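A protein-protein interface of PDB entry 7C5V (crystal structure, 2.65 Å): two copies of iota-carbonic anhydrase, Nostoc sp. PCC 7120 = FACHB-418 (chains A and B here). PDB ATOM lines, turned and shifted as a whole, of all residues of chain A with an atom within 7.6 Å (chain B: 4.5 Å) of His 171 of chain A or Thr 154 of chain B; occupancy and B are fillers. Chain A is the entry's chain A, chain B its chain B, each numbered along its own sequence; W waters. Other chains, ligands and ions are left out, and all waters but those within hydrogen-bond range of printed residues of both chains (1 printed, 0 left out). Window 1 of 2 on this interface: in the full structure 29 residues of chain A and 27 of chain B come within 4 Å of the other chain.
N of Phe 76 of chain A is in hydrogen-bond range of SD of Met 136 of chain B, 3.8 Å away.
N of Lys 77 of chain A lies close to SD of Met 136 of chain B, 3.6 Å away.
NZ of Lys 77 of chain A lies within salt-bridge range of OD2 of Asp 152 of chain B (3.97 Å).
The side-chain amide nitrogen (NE2) of Gln 156 of chain B sits at hydrogen-bond distance from the side-chain hydroxyl (OG1) of Thr 134 of chain A, at 2.7 Å.
A ring nitrogen (ND1) of His 171 of chain B lies within hydrogen-bond range of the side-chain hydroxyl of Thr 154 of chain A (2.7 Å).
The side-chain amide nitrogen (NE2) of Gln 156 of chain A lies within hydrogen-bond range of the side-chain hydroxyl (OG1) of Thr 134 of chain B (2.8 Å).
The side-chain amide oxygen (OE1) of Gln 156 of chain B lies close to the side-chain amide oxygen (OE1) of Gln 156 of chain A (3.4 Å).
The side-chain hydroxyl (OG1) of Thr 154 of chain B lies within hydrogen-bond range of a ring nitrogen (ND1) of His 171 of chain A.
The side-chain hydroxyl (OG) of Ser 173 of chain B is in hydrogen-bond range of a ring nitrogen (NE2) of His 171 of chain A, 2.7 Å away.
The side-chain hydroxyl (OG) of Ser 173 of chain A lies within hydrogen-bond range of a ring nitrogen (NE2) of His 171 of chain B (2.8 Å).
The backbone carbonyl oxygen of Leu 75 of chain A sits close to the side-chain sulfur of Met 136 of chain B (3.6 Å).
The side-chain amide nitrogen (NE2) of Gln 156 of chain A lies within hydrogen-bond range of the side-chain hydroxyl (OG1) of Thr 169 of chain A, 2.6 Å away.
N of Asp 152 of chain B is in hydrogen-bond range of O of Ser 173 of chain B, 2.9 Å away.
N of Thr 154 of chain B lies within hydrogen-bond range of O of His 171 of chain B (2.9 Å).
Water W1 lies within hydrogen-bond range of NZ of Lys 77 of chain A (2.5 Å), OD2 of Asp 152 of chain B (2.6 Å) and OG of Ser 173 of chain B (2.9 Å).
Leu 75 of chain A touches Thr 134 of chain B (CD2 to O, 3.5 Å).
Leu 75 of chain A touches Thr 135 of chain B.
His 171 of chain B touches Met 136 of chain A.
His 171 of chain B touches Asp 152 of chain A (CE1 to O, 3.1 Å).
Thr 154 of chain B touches Thr 169 of chain A (CG2 to CG2, 3.8 Å).
CE of Met 136 of chain B touches CB of His 171 of chain A, 3.98 Å away.
Of the printed residues of chain B, His 171 of chain A touches Met 136, Asp 152, Thr 154, His 171 and Ser 173.
Thr 154 of chain B touches just these residues of chain A: Thr 169 (3.8 Å) and His 171 (2.6 Å).
Printed residues of chain B within 4 Å of Lys 77 of chain A: Met 136, Asp 152 and Ser 173.
Of the printed residues of chain B, Met 136 of chain A touches His 171.
The nearest printed residue of chain B that does not touch His 171 of chain A is Lys 153 of chain B (4.1 Å).
The nearest printed residue of chain A that does not touch Thr 154 of chain B is Thr 154 of chain A (5.2 Å).
The nearest printed residue of chain A that does not touch Met 136 of chain B is His 170 of chain A (4.2 Å).
Of the 24 printed residues of chain A, 13 touch a printed residue of chain B.
Hydrophobic or aromatic side chains of chain A that line the printed part of chain B: Leu 75, Phe 87, Met 136 and His 171.
Of the 12 printed residues of chain B, 9 touch a printed residue of chain A.
Hydrophobic or aromatic side chains of chain B that line the printed part of chain A: Met 136 and His 171.
Among the printed residues, Asp or Glu carboxylates within 4 Å of a Lys or Arg side-chain nitrogen of the other chain: Lys 77 of chain A with Asp 152 of chain B.
Thr 134 of chain A touches Gln 156 of chain B, and with the chains exchanged Gln 156 of chain A touches Thr 134 of chain B.
Ser 173 of chain A touches its own counterpart, Ser 173 of chain B.
Of the 27 pairs that touch across the chains among the printed residues, 17 have their exchanged pair printed and touching as well.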
ATOM      1  N   LEU A  75      10.956  24.141  28.981  1.00  0.00           N
ATOM      2  CA  LEU A  75      12.359  23.726  28.920  1.00  0.00           C
ATOM      3  C   LEU A  75      13.043  24.303  30.163  1.00  0.00           C
ATOM      4  O   LEU A  75      13.704  25.345  30.141  1.00  0.00           O
ATOM      5  CB  LEU A  75      12.995  24.184  27.608  1.00  0.00           C
ATOM      6  CG  LEU A  75      12.610  23.486  26.283  1.00  0.00           C
ATOM      7  CD1 LEU A  75      11.159  23.583  25.940  1.00  0.00           C
ATOM      8  CD2 LEU A  75      13.428  24.040  25.119  1.00  0.00           C
ATOM      9  N   PHE A  76      12.811  23.637  31.293  1.00  0.00           N
ATOM     10  CA  PHE A  76      13.280  24.084  32.601  1.00  0.00           C
ATOM     11  C   PHE A  76      14.406  23.159  33.035  1.00  0.00           C
ATOM     12  O   PHE A  76      14.170  21.976  33.301  1.00  0.00           O
ATOM     13  CB  PHE A  76      12.136  24.076  33.617  1.00  0.00           C
ATOM     14  CG  PHE A  76      12.475  24.735  34.946  1.00  0.00           C
ATOM     15  CD1 PHE A  76      13.619  25.509  35.100  1.00  0.00           C
ATOM     16  CD2 PHE A  76      11.646  24.568  36.047  1.00  0.00           C
ATOM     17  CE1 PHE A  76      13.913  26.106  36.336  1.00  0.00           C
ATOM     18  CE2 PHE A  76      11.945  25.156  37.270  1.00  0.00           C
ATOM     19  CZ  PHE A  76      13.067  25.921  37.414  1.00  0.00           C
ATOM     20  N   LYS A  77      15.630  23.680  33.065  1.00  0.00           N
ATOM     21  CA  LYS A  77      16.775  22.949  33.610  1.00  0.00           C
ATOM     22  C   LYS A  77      17.258  23.766  34.799  1.00  0.00           C
ATOM     23  O   LYS A  77      17.911  24.813  34.619  1.00  0.00           O
ATOM     24  CB  LYS A  77      17.884  22.735  32.585  1.00  0.00           C
ATOM     25  CG  LYS A  77      19.081  21.969  33.149  1.00  0.00           C
ATOM     26  CD  LYS A  77      20.082  22.910  33.760  1.00  0.00           C
ATOM     27  CE  LYS A  77      20.996  22.250  34.711  1.00  0.00           C
ATOM     28  NZ  LYS A  77      22.162  23.138  34.977  1.00  0.00           N
ATOM     29  N   PRO A  78      16.948  23.342  36.022  1.00  0.00           N
ATOM     30  CA  PRO A  78      17.248  24.162  37.198  1.00  0.00           C
ATOM     31  C   PRO A  78      18.702  24.026  37.625  1.00  0.00           C
ATOM     32  O   PRO A  78      19.410  23.103  37.227  1.00  0.00           O
ATOM     33  CB  PRO A  78      16.297  23.601  38.265  1.00  0.00           C
ATOM     34  CG  PRO A  78      15.291  22.755  37.493  1.00  0.00           C
ATOM     35  CD  PRO A  78      16.077  22.205  36.360  1.00  0.00           C
ATOM     36  N   THR A  79      19.143  24.982  38.449  1.00  0.00           N
ATOM     37  CA  THR A  79      20.560  25.054  38.814  1.00  0.00           C
ATOM     38  C   THR A  79      21.086  23.721  39.342  1.00  0.00           C
ATOM     39  O   THR A  79      22.137  23.237  38.897  1.00  0.00           O
ATOM     40  CB  THR A  79      20.784  26.143  39.860  1.00  0.00           C
ATOM     41  OG1 THR A  79      20.012  27.301  39.526  1.00  0.00           O
ATOM     42  CG2 THR A  79      22.239  26.512  39.905  1.00  0.00           C
ATOM     43  N   THR A  86      17.145  15.890  35.439  1.00  0.00           N
ATOM     44  CA  THR A  86      17.797  17.149  35.099  1.00  0.00           C
ATOM     45  C   THR A  86      16.791  18.161  34.566  1.00  0.00           C
ATOM     46  O   THR A  86      16.811  19.338  34.951  1.00  0.00           O
ATOM     47  CB  THR A  86      18.884  16.905  34.055  1.00  0.00           C
ATOM     48  OG1 THR A  86      19.901  16.058  34.590  1.00  0.00           O
ATOM     49  CG2 THR A  86      19.497  18.219  33.618  1.00  0.00           C
ATOM     50  N   PHE A  87      15.896  17.718  33.695  1.00  0.00           N
ATOM     51  CA  PHE A  87      15.005  18.608  32.967  1.00  0.00           C
ATOM     52  C   PHE A  87      13.602  18.497  33.539  1.00  0.00           C
ATOM     53  O   PHE A  87      13.028  17.406  33.567  1.00  0.00           O
ATOM     54  CB  PHE A  87      15.051  18.270  31.480  1.00  0.00           C
ATOM     55  CG  PHE A  87      16.453  18.224  30.940  1.00  0.00           C
ATOM     56  CD1 PHE A  87      17.186  19.402  30.799  1.00  0.00           C
ATOM     57  CD2 PHE A  87      17.053  17.017  30.628  1.00  0.00           C
ATOM     58  CE1 PHE A  87      18.485  19.398  30.315  1.00  0.00           C
ATOM     59  CE2 PHE A  87      18.348  16.988  30.148  1.00  0.00           C
ATOM     60  CZ  PHE A  87      19.073  18.191  29.979  1.00  0.00           C
ATOM     61  N   THR A 134      14.296  36.248  24.445  1.00  0.00           N
ATOM     62  CA  THR A 134      15.261  35.516  25.252  1.00  0.00           C
ATOM     63  C   THR A 134      16.190  36.495  25.947  1.00  0.00           C
ATOM     64  O   THR A 134      16.645  37.470  25.345  1.00  0.00           O
ATOM     65  CB  THR A 134      16.083  34.540  24.409  1.00  0.00           C
ATOM     66  OG1 THR A 134      15.209  33.702  23.651  1.00  0.00           O
ATOM     67  CG2 THR A 134      16.950  33.662  25.298  1.00  0.00           C
ATOM     68  N   THR A 135      16.462  36.238  27.219  1.00  0.00           N
ATOM     69  CA  THR A 135      17.503  36.948  27.941  1.00  0.00           C
ATOM     70  C   THR A 135      18.557  35.963  28.415  1.00  0.00           C
ATOM     71  O   THR A 135      18.258  34.799  28.711  1.00  0.00           O
ATOM     72  CB  THR A 135      16.952  37.679  29.141  1.00  0.00           C
ATOM     73  OG1 THR A 135      16.614  36.703  30.122  1.00  0.00           O
ATOM     74  CG2 THR A 135      15.720  38.478  28.766  1.00  0.00           C
ATOM     75  N   MET A 136      19.802  36.435  28.481  1.00  0.00           N
ATOM     76  CA  MET A 136      20.872  35.663  29.092  1.00  0.00           C
ATOM     77  C   MET A 136      21.756  36.621  29.865  1.00  0.00           C
ATOM     78  O   MET A 136      22.066  37.713  29.384  1.00  0.00           O
ATOM     79  CB  MET A 136      21.687  34.892  28.057  1.00  0.00           C
ATOM     80  CG  MET A 136      23.001  34.388  28.608  1.00  0.00           C
ATOM     81  SD  MET A 136      23.965  33.522  27.373  1.00  0.00           S
ATOM     82  CE  MET A 136      23.054  32.012  27.194  1.00  0.00           C
ATOM     83  N   GLY A 137      22.123  36.225  31.073  1.00  0.00           N
ATOM     84  CA  GLY A 137      22.925  37.056  31.949  1.00  0.00           C
ATOM     85  C   GLY A 137      23.052  36.411  33.317  1.00  0.00           C
ATOM     86  O   GLY A 137      22.974  35.181  33.436  1.00  0.00           O
ATOM     87  N   VAL A 151      23.942  32.886  39.610  1.00  0.00           N
ATOM     88  CA  VAL A 151      23.711  31.859  38.596  1.00  0.00           C
ATOM     89  C   VAL A 151      23.792  32.501  37.224  1.00  0.00           C
ATOM     90  O   VAL A 151      23.557  33.702  37.070  1.00  0.00           O
ATOM     91  CB  VAL A 151      22.349  31.152  38.771  1.00  0.00           C
ATOM     92  CG1 VAL A 151      22.328  30.357  40.072  1.00  0.00           C
ATOM     93  CG2 VAL A 151      21.204  32.176  38.719  1.00  0.00           C
ATOM     94  N   ASP A 152      24.158  31.693  36.228  1.00  0.00           N
ATOM     95  CA  ASP A 152      24.051  32.062  34.821  1.00  0.00           C
ATOM     96  C   ASP A 152      22.696  31.587  34.309  1.00  0.00           C
ATOM     97  O   ASP A 152      22.416  30.390  34.333  1.00  0.00           O
ATOM     98  CB  ASP A 152      25.173  31.424  34.002  1.00  0.00           C
ATOM     99  CG  ASP A 152      26.556  31.792  34.503  1.00  0.00           C
ATOM    100  OD1 ASP A 152      26.729  32.927  34.983  1.00  0.00           O
ATOM    101  OD2 ASP A 152      27.475  30.953  34.405  1.00  0.00           O
ATOM    102  N   LYS A 153      21.853  32.506  33.847  1.00  0.00           N
ATOM    103  CA  LYS A 153      20.488  32.130  33.509  1.00  0.00           C
ATOM    104  C   LYS A 153      20.111  32.549  32.094  1.00  0.00           C
ATOM    105  O   LYS A 153      20.441  33.650  31.641  1.00  0.00           O
ATOM    106  CB  LYS A 153      19.497  32.732  34.489  1.00  0.00           C
ATOM    107  CG  LYS A 153      18.199  31.966  34.556  1.00  0.00           C
ATOM    108  CD  LYS A 153      17.317  32.569  35.616  1.00  0.00           C
ATOM    109  CE  LYS A 153      17.923  32.416  36.986  1.00  0.00           C
ATOM    110  NZ  LYS A 153      17.535  31.108  37.549  1.00  0.00           N
ATOM    111  N   THR A 154      19.404  31.653  31.412  1.00  0.00           N
ATOM    112  CA  THR A 154      18.757  31.935  30.148  1.00  0.00           C
ATOM    113  C   THR A 154      17.261  31.770  30.340  1.00  0.00           C
ATOM    114  O   THR A 154      16.806  30.728  30.832  1.00  0.00           O
ATOM    115  CB  THR A 154      19.240  30.997  29.066  1.00  0.00           C
ATOM    116  OG1 THR A 154      20.619  31.260  28.819  1.00  0.00           O
ATOM    117  CG2 THR A 154      18.451  31.232  27.810  1.00  0.00           C
ATOM    118  N   TRP A 155      16.508  32.804  29.985  1.00  0.00           N
ATOM    119  CA  TRP A 155      15.060  32.786  30.044  1.00  0.00           C
ATOM    120  C   TRP A 155      14.507  32.955  28.640  1.00  0.00           C
ATOM    121  O   TRP A 155      15.097  33.640  27.800  1.00  0.00           O
ATOM    122  CB  TRP A 155      14.529  33.909  30.932  1.00  0.00           C
ATOM    123  CG  TRP A 155      14.291  33.524  32.361  1.00  0.00           C
ATOM    124  CD1 TRP A 155      13.733  32.367  32.822  1.00  0.00           C
ATOM    125  CD2 TRP A 155      14.593  34.314  33.519  1.00  0.00           C
ATOM    126  NE1 TRP A 155      13.666  32.387  34.191  1.00  0.00           N
ATOM    127  CE2 TRP A 155      14.186  33.571  34.646  1.00  0.00           C
ATOM    128  CE3 TRP A 155      15.164  35.581  33.711  1.00  0.00           C
ATOM    129  CZ2 TRP A 155      14.329  34.048  35.947  1.00  0.00           C
ATOM    130  CZ3 TRP A 155      15.317  36.050  34.997  1.00  0.00           C
ATOM    131  CH2 TRP A 155      14.897  35.284  36.104  1.00  0.00           C
ATOM    132  N   GLN A 156      13.376  32.325  28.378  1.00  0.00           N
ATOM    133  CA  GLN A 156      12.623  32.629  27.174  1.00  0.00           C
ATOM    134  C   GLN A 156      11.205  32.949  27.603  1.00  0.00           C
ATOM    135  O   GLN A 156      10.611  32.195  28.380  1.00  0.00           O
ATOM    136  CB  GLN A 156      12.637  31.482  26.160  1.00  0.00           C
ATOM    137  CG  GLN A 156      12.632  31.941  24.719  1.00  0.00           C
ATOM    138  CD  GLN A 156      12.412  30.812  23.729  1.00  0.00           C
ATOM    139  OE1 GLN A 156      12.080  31.057  22.563  1.00  0.00           O
ATOM    140  NE2 GLN A 156      12.602  29.577  24.173  1.00  0.00           N
ATOM    141  N   ILE A 167       7.204  31.989  30.842  1.00  0.00           N
ATOM    142  CA  ILE A 167       8.513  31.362  30.693  1.00  0.00           C
ATOM    143  C   ILE A 167       8.340  29.993  30.053  1.00  0.00           C
ATOM    144  O   ILE A 167       7.729  29.087  30.634  1.00  0.00           O
ATOM    145  CB  ILE A 167       9.236  31.245  32.040  1.00  0.00           C
ATOM    146  CG1 ILE A 167       9.491  32.631  32.633  1.00  0.00           C
ATOM    147  CG2 ILE A 167      10.526  30.430  31.881  1.00  0.00           C
ATOM    148  CD1 ILE A 167       9.858  32.594  34.098  1.00  0.00           C
ATOM    149  N   THR A 169      11.294  28.648  28.582  1.00  0.00           N
ATOM    150  CA  THR A 169      12.656  28.149  28.675  1.00  0.00           C
ATOM    151  C   THR A 169      13.335  28.771  29.879  1.00  0.00           C
ATOM    152  O   THR A 169      13.220  29.974  30.105  1.00  0.00           O
ATOM    153  CB  THR A 169      13.487  28.485  27.440  1.00  0.00           C
ATOM    154  OG1 THR A 169      12.805  28.037  26.267  1.00  0.00           O
ATOM    155  CG2 THR A 169      14.871  27.833  27.529  1.00  0.00           C
ATOM    156  N   HIS A 170      14.087  27.957  30.620  1.00  0.00           N
ATOM    157  CA  HIS A 170      14.688  28.420  31.869  1.00  0.00           C
ATOM    158  C   HIS A 170      15.904  27.533  32.154  1.00  0.00           C
ATOM    159  O   HIS A 170      15.799  26.501  32.829  1.00  0.00           O
ATOM    160  CB  HIS A 170      13.660  28.380  32.990  1.00  0.00           C
ATOM    161  CG  HIS A 170      14.135  28.940  34.297  1.00  0.00           C
ATOM    162  ND1 HIS A 170      15.466  29.138  34.596  1.00  0.00           N
ATOM    163  CD2 HIS A 170      13.442  29.341  35.391  1.00  0.00           C
ATOM    164  CE1 HIS A 170      15.572  29.641  35.813  1.00  0.00           C
ATOM    165  NE2 HIS A 170      14.357  29.772  36.317  1.00  0.00           N
ATOM    166  N   HIS A 171      17.053  27.951  31.634  1.00  0.00           N
ATOM    167  CA  HIS A 171      18.308  27.247  31.854  1.00  0.00           C
ATOM    168  C   HIS A 171      19.113  27.994  32.907  1.00  0.00           C
ATOM    169  O   HIS A 171      19.525  29.129  32.682  1.00  0.00           O
ATOM    170  CB  HIS A 171      19.092  27.126  30.554  1.00  0.00           C
ATOM    171  CG  HIS A 171      20.211  26.140  30.622  1.00  0.00           C
ATOM    172  ND1 HIS A 171      20.598  25.371  29.543  1.00  0.00           N
ATOM    173  CD2 HIS A 171      21.030  25.795  31.641  1.00  0.00           C
ATOM    174  CE1 HIS A 171      21.619  24.612  29.890  1.00  0.00           C
ATOM    175  NE2 HIS A 171      21.894  24.843  31.161  1.00  0.00           N
ATOM    176  N   SER A 172      19.311  27.368  34.061  1.00  0.00           N
ATOM    177  CA  SER A 172      20.115  27.924  35.141  1.00  0.00           C
ATOM    178  C   SER A 172      21.334  27.034  35.360  1.00  0.00           C
ATOM    179  O   SER A 172      21.260  25.814  35.181  1.00  0.00           O
ATOM    180  CB  SER A 172      19.288  28.030  36.425  1.00  0.00           C
ATOM    181  OG  SER A 172      19.651  29.147  37.210  1.00  0.00           O
ATOM    182  N   SER A 173      22.460  27.630  35.745  1.00  0.00           N
ATOM    183  CA  SER A 173      23.663  26.834  35.965  1.00  0.00           C
ATOM    184  C   SER A 173      24.598  27.547  36.927  1.00  0.00           C
ATOM    185  O   SER A 173      24.657  28.779  36.966  1.00  0.00           O
ATOM    186  CB  SER A 173      24.395  26.544  34.650  1.00  0.00           C
ATOM    187  OG  SER A 173      24.688  27.722  33.912  1.00  0.00           O
ATOM    188  N   LEU A 174      25.331  26.761  37.699  1.00  0.00           N
ATOM    189  CA  LEU A 174      26.385  27.330  38.532  1.00  0.00           C
ATOM    190  C   LEU A 174      27.515  27.838  37.638  1.00  0.00           C
ATOM    191  O   LEU A 174      27.909  27.145  36.688  1.00  0.00           O
ATOM    192  CB  LEU A 174      26.908  26.288  39.518  1.00  0.00           C
ATOM    193  CG  LEU A 174      25.898  25.728  40.523  1.00  0.00           C
ATOM    194  CD1 LEU A 174      26.500  24.574  41.286  1.00  0.00           C
ATOM    195  CD2 LEU A 174      25.428  26.805  41.480  1.00  0.00           C
ATOM    196  N   THR B 134      13.553  26.273  19.908  1.00  0.00           N
ATOM    197  CA  THR B 134      14.396  26.045  21.083  1.00  0.00           C
ATOM    198  C   THR B 134      14.403  24.567  21.451  1.00  0.00           C
ATOM    199  O   THR B 134      13.339  23.951  21.600  1.00  0.00           O
ATOM    200  CB  THR B 134      13.927  26.860  22.301  1.00  0.00           C
ATOM    201  OG1 THR B 134      13.538  28.173  21.902  1.00  0.00           O
ATOM    202  CG2 THR B 134      15.031  26.982  23.325  1.00  0.00           C
ATOM    203  N   THR B 135      15.597  24.009  21.616  1.00  0.00           N
ATOM    204  CA  THR B 135      15.773  22.679  22.169  1.00  0.00           C
ATOM    205  C   THR B 135      16.455  22.779  23.525  1.00  0.00           C
ATOM    206  O   THR B 135      17.272  23.676  23.764  1.00  0.00           O
ATOM    207  CB  THR B 135      16.617  21.792  21.252  1.00  0.00           C
ATOM    208  OG1 THR B 135      17.998  22.160  21.369  1.00  0.00           O
ATOM    209  CG2 THR B 135      16.172  21.921  19.812  1.00  0.00           C
ATOM    210  N   MET B 136      16.108  21.851  24.413  1.00  0.00           N
ATOM    211  CA  MET B 136      16.827  21.633  25.662  1.00  0.00           C
ATOM    212  C   MET B 136      17.017  20.141  25.839  1.00  0.00           C
ATOM    213  O   MET B 136      16.072  19.367  25.666  1.00  0.00           O
ATOM    214  CB  MET B 136      16.091  22.201  26.884  1.00  0.00           C
ATOM    215  CG  MET B 136      16.749  21.808  28.216  1.00  0.00           C
ATOM    216  SD  MET B 136      16.068  22.679  29.644  1.00  0.00           S
ATOM    217  CE  MET B 136      16.491  24.386  29.292  1.00  0.00           C
ATOM    218  N   ASP B 152      24.563  19.694  29.697  1.00  0.00           N
ATOM    219  CA  ASP B 152      23.192  20.177  29.594  1.00  0.00           C
ATOM    220  C   ASP B 152      23.170  21.376  28.649  1.00  0.00           C
ATOM    221  O   ASP B 152      23.926  22.338  28.848  1.00  0.00           O
ATOM    222  CB  ASP B 152      22.679  20.578  30.973  1.00  0.00           C
ATOM    223  CG  ASP B 152      22.628  19.410  31.941  1.00  0.00           C
ATOM    224  OD1 ASP B 152      22.548  18.265  31.466  1.00  0.00           O
ATOM    225  OD2 ASP B 152      22.663  19.643  33.166  1.00  0.00           O
ATOM    226  N   LYS B 153      22.322  21.327  27.621  1.00  0.00           N
ATOM    227  CA  LYS B 153      22.415  22.295  26.534  1.00  0.00           C
ATOM    228  C   LYS B 153      21.052  22.855  26.153  1.00  0.00           C
ATOM    229  O   LYS B 153      20.076  22.109  26.031  1.00  0.00           O
ATOM    230  CB  LYS B 153      23.073  21.673  25.293  1.00  0.00           C
ATOM    231  CG  LYS B 153      23.615  22.732  24.360  1.00  0.00           C
ATOM    232  CD  LYS B 153      24.377  22.164  23.192  1.00  0.00           C
ATOM    233  CE  LYS B 153      25.736  21.670  23.586  1.00  0.00           C
ATOM    234  NZ  LYS B 153      26.631  22.767  24.010  1.00  0.00           N
ATOM    235  N   THR B 154      20.998  24.173  25.945  1.00  0.00           N
ATOM    236  CA  THR B 154      19.845  24.855  25.363  1.00  0.00           C
ATOM    237  C   THR B 154      20.302  25.573  24.097  1.00  0.00           C
ATOM    238  O   THR B 154      21.241  26.379  24.140  1.00  0.00           O
ATOM    239  CB  THR B 154      19.238  25.857  26.343  1.00  0.00           C
ATOM    240  OG1 THR B 154      18.916  25.187  27.564  1.00  0.00           O
ATOM    241  CG2 THR B 154      17.965  26.505  25.760  1.00  0.00           C
ATOM    242  N   TRP B 155      19.650  25.270  22.972  1.00  0.00           N
ATOM    243  CA  TRP B 155      19.916  25.910  21.696  1.00  0.00           C
ATOM    244  C   TRP B 155      18.669  26.655  21.262  1.00  0.00           C
ATOM    245  O   TRP B 155      17.553  26.139  21.402  1.00  0.00           O
ATOM    246  CB  TRP B 155      20.264  24.898  20.618  1.00  0.00           C
ATOM    247  CG  TRP B 155      21.699  24.629  20.439  1.00  0.00           C
ATOM    248  CD1 TRP B 155      22.711  25.543  20.392  1.00  0.00           C
ATOM    249  CD2 TRP B 155      22.314  23.335  20.272  1.00  0.00           C
ATOM    250  NE1 TRP B 155      23.924  24.895  20.218  1.00  0.00           N
ATOM    251  CE2 TRP B 155      23.700  23.544  20.134  1.00  0.00           C
ATOM    252  CE3 TRP B 155      21.822  22.024  20.230  1.00  0.00           C
ATOM    253  CZ2 TRP B 155      24.594  22.490  19.937  1.00  0.00           C
ATOM    254  CZ3 TRP B 155      22.713  20.982  20.047  1.00  0.00           C
ATOM    255  CH2 TRP B 155      24.079  21.217  19.901  1.00  0.00           C
ATOM    256  N   GLN B 156      18.850  27.857  20.721  1.00  0.00           N
ATOM    257  CA  GLN B 156      17.784  28.530  19.988  1.00  0.00           C
ATOM    258  C   GLN B 156      18.263  28.833  18.575  1.00  0.00           C
ATOM    259  O   GLN B 156      19.339  29.409  18.380  1.00  0.00           O
ATOM    260  CB  GLN B 156      17.304  29.811  20.686  1.00  0.00           C
ATOM    261  CG  GLN B 156      16.091  30.409  20.018  1.00  0.00           C
ATOM    262  CD  GLN B 156      15.517  31.630  20.734  1.00  0.00           C
ATOM    263  OE1 GLN B 156      14.445  32.126  20.362  1.00  0.00           O
ATOM    264  NE2 GLN B 156      16.223  32.123  21.750  1.00  0.00           N
ATOM    265  N   THR B 169      20.891  31.511  20.609  1.00  0.00           N
ATOM    266  CA  THR B 169      21.111  31.206  22.023  1.00  0.00           C
ATOM    267  C   THR B 169      21.821  29.866  22.154  1.00  0.00           C
ATOM    268  O   THR B 169      21.489  28.907  21.447  1.00  0.00           O
ATOM    269  CB  THR B 169      19.801  31.166  22.803  1.00  0.00           C
ATOM    270  OG1 THR B 169      19.094  32.391  22.581  1.00  0.00           O
ATOM    271  CG2 THR B 169      20.052  30.995  24.305  1.00  0.00           C
ATOM    272  N   HIS B 170      22.794  29.811  23.072  1.00  0.00           N
ATOM    273  CA  HIS B 170      23.627  28.623  23.286  1.00  0.00           C
ATOM    274  C   HIS B 170      24.095  28.644  24.743  1.00  0.00           C
ATOM    275  O   HIS B 170      25.130  29.233  25.071  1.00  0.00           O
ATOM    276  CB  HIS B 170      24.786  28.615  22.300  1.00  0.00           C
ATOM    277  CG  HIS B 170      25.641  27.384  22.336  1.00  0.00           C
ATOM    278  ND1 HIS B 170      25.728  26.553  23.435  1.00  0.00           N
ATOM    279  CD2 HIS B 170      26.482  26.866  21.408  1.00  0.00           C
ATOM    280  CE1 HIS B 170      26.582  25.576  23.182  1.00  0.00           C
ATOM    281  NE2 HIS B 170      27.046  25.738  21.954  1.00  0.00           N
ATOM    282  N   HIS B 171      23.313  28.009  25.612  1.00  0.00           N
ATOM    283  CA  HIS B 171      23.635  27.880  27.034  1.00  0.00           C
ATOM    284  C   HIS B 171      24.068  26.450  27.283  1.00  0.00           C
ATOM    285  O   HIS B 171      23.283  25.523  27.075  1.00  0.00           O
ATOM    286  CB  HIS B 171      22.433  28.231  27.910  1.00  0.00           C
ATOM    287  CG  HIS B 171      22.766  28.458  29.355  1.00  0.00           C
ATOM    288  ND1 HIS B 171      22.142  29.423  30.119  1.00  0.00           N
ATOM    289  CD2 HIS B 171      23.627  27.827  30.187  1.00  0.00           C
ATOM    290  CE1 HIS B 171      22.614  29.388  31.354  1.00  0.00           C
ATOM    291  NE2 HIS B 171      23.514  28.426  31.422  1.00  0.00           N
ATOM    292  N   SER B 173      26.043  23.801  30.130  1.00  0.00           N
ATOM    293  CA  SER B 173      26.525  23.681  31.497  1.00  0.00           C
ATOM    294  C   SER B 173      26.883  22.242  31.848  1.00  0.00           C
ATOM    295  O   SER B 173      26.351  21.278  31.281  1.00  0.00           O
ATOM    296  CB  SER B 173      25.523  24.274  32.501  1.00  0.00           C
ATOM    297  OG  SER B 173      24.203  23.937  32.191  1.00  0.00           O
HETATM  298  O   HOH W   1      23.990  21.711  34.088  1.00  0.00           O
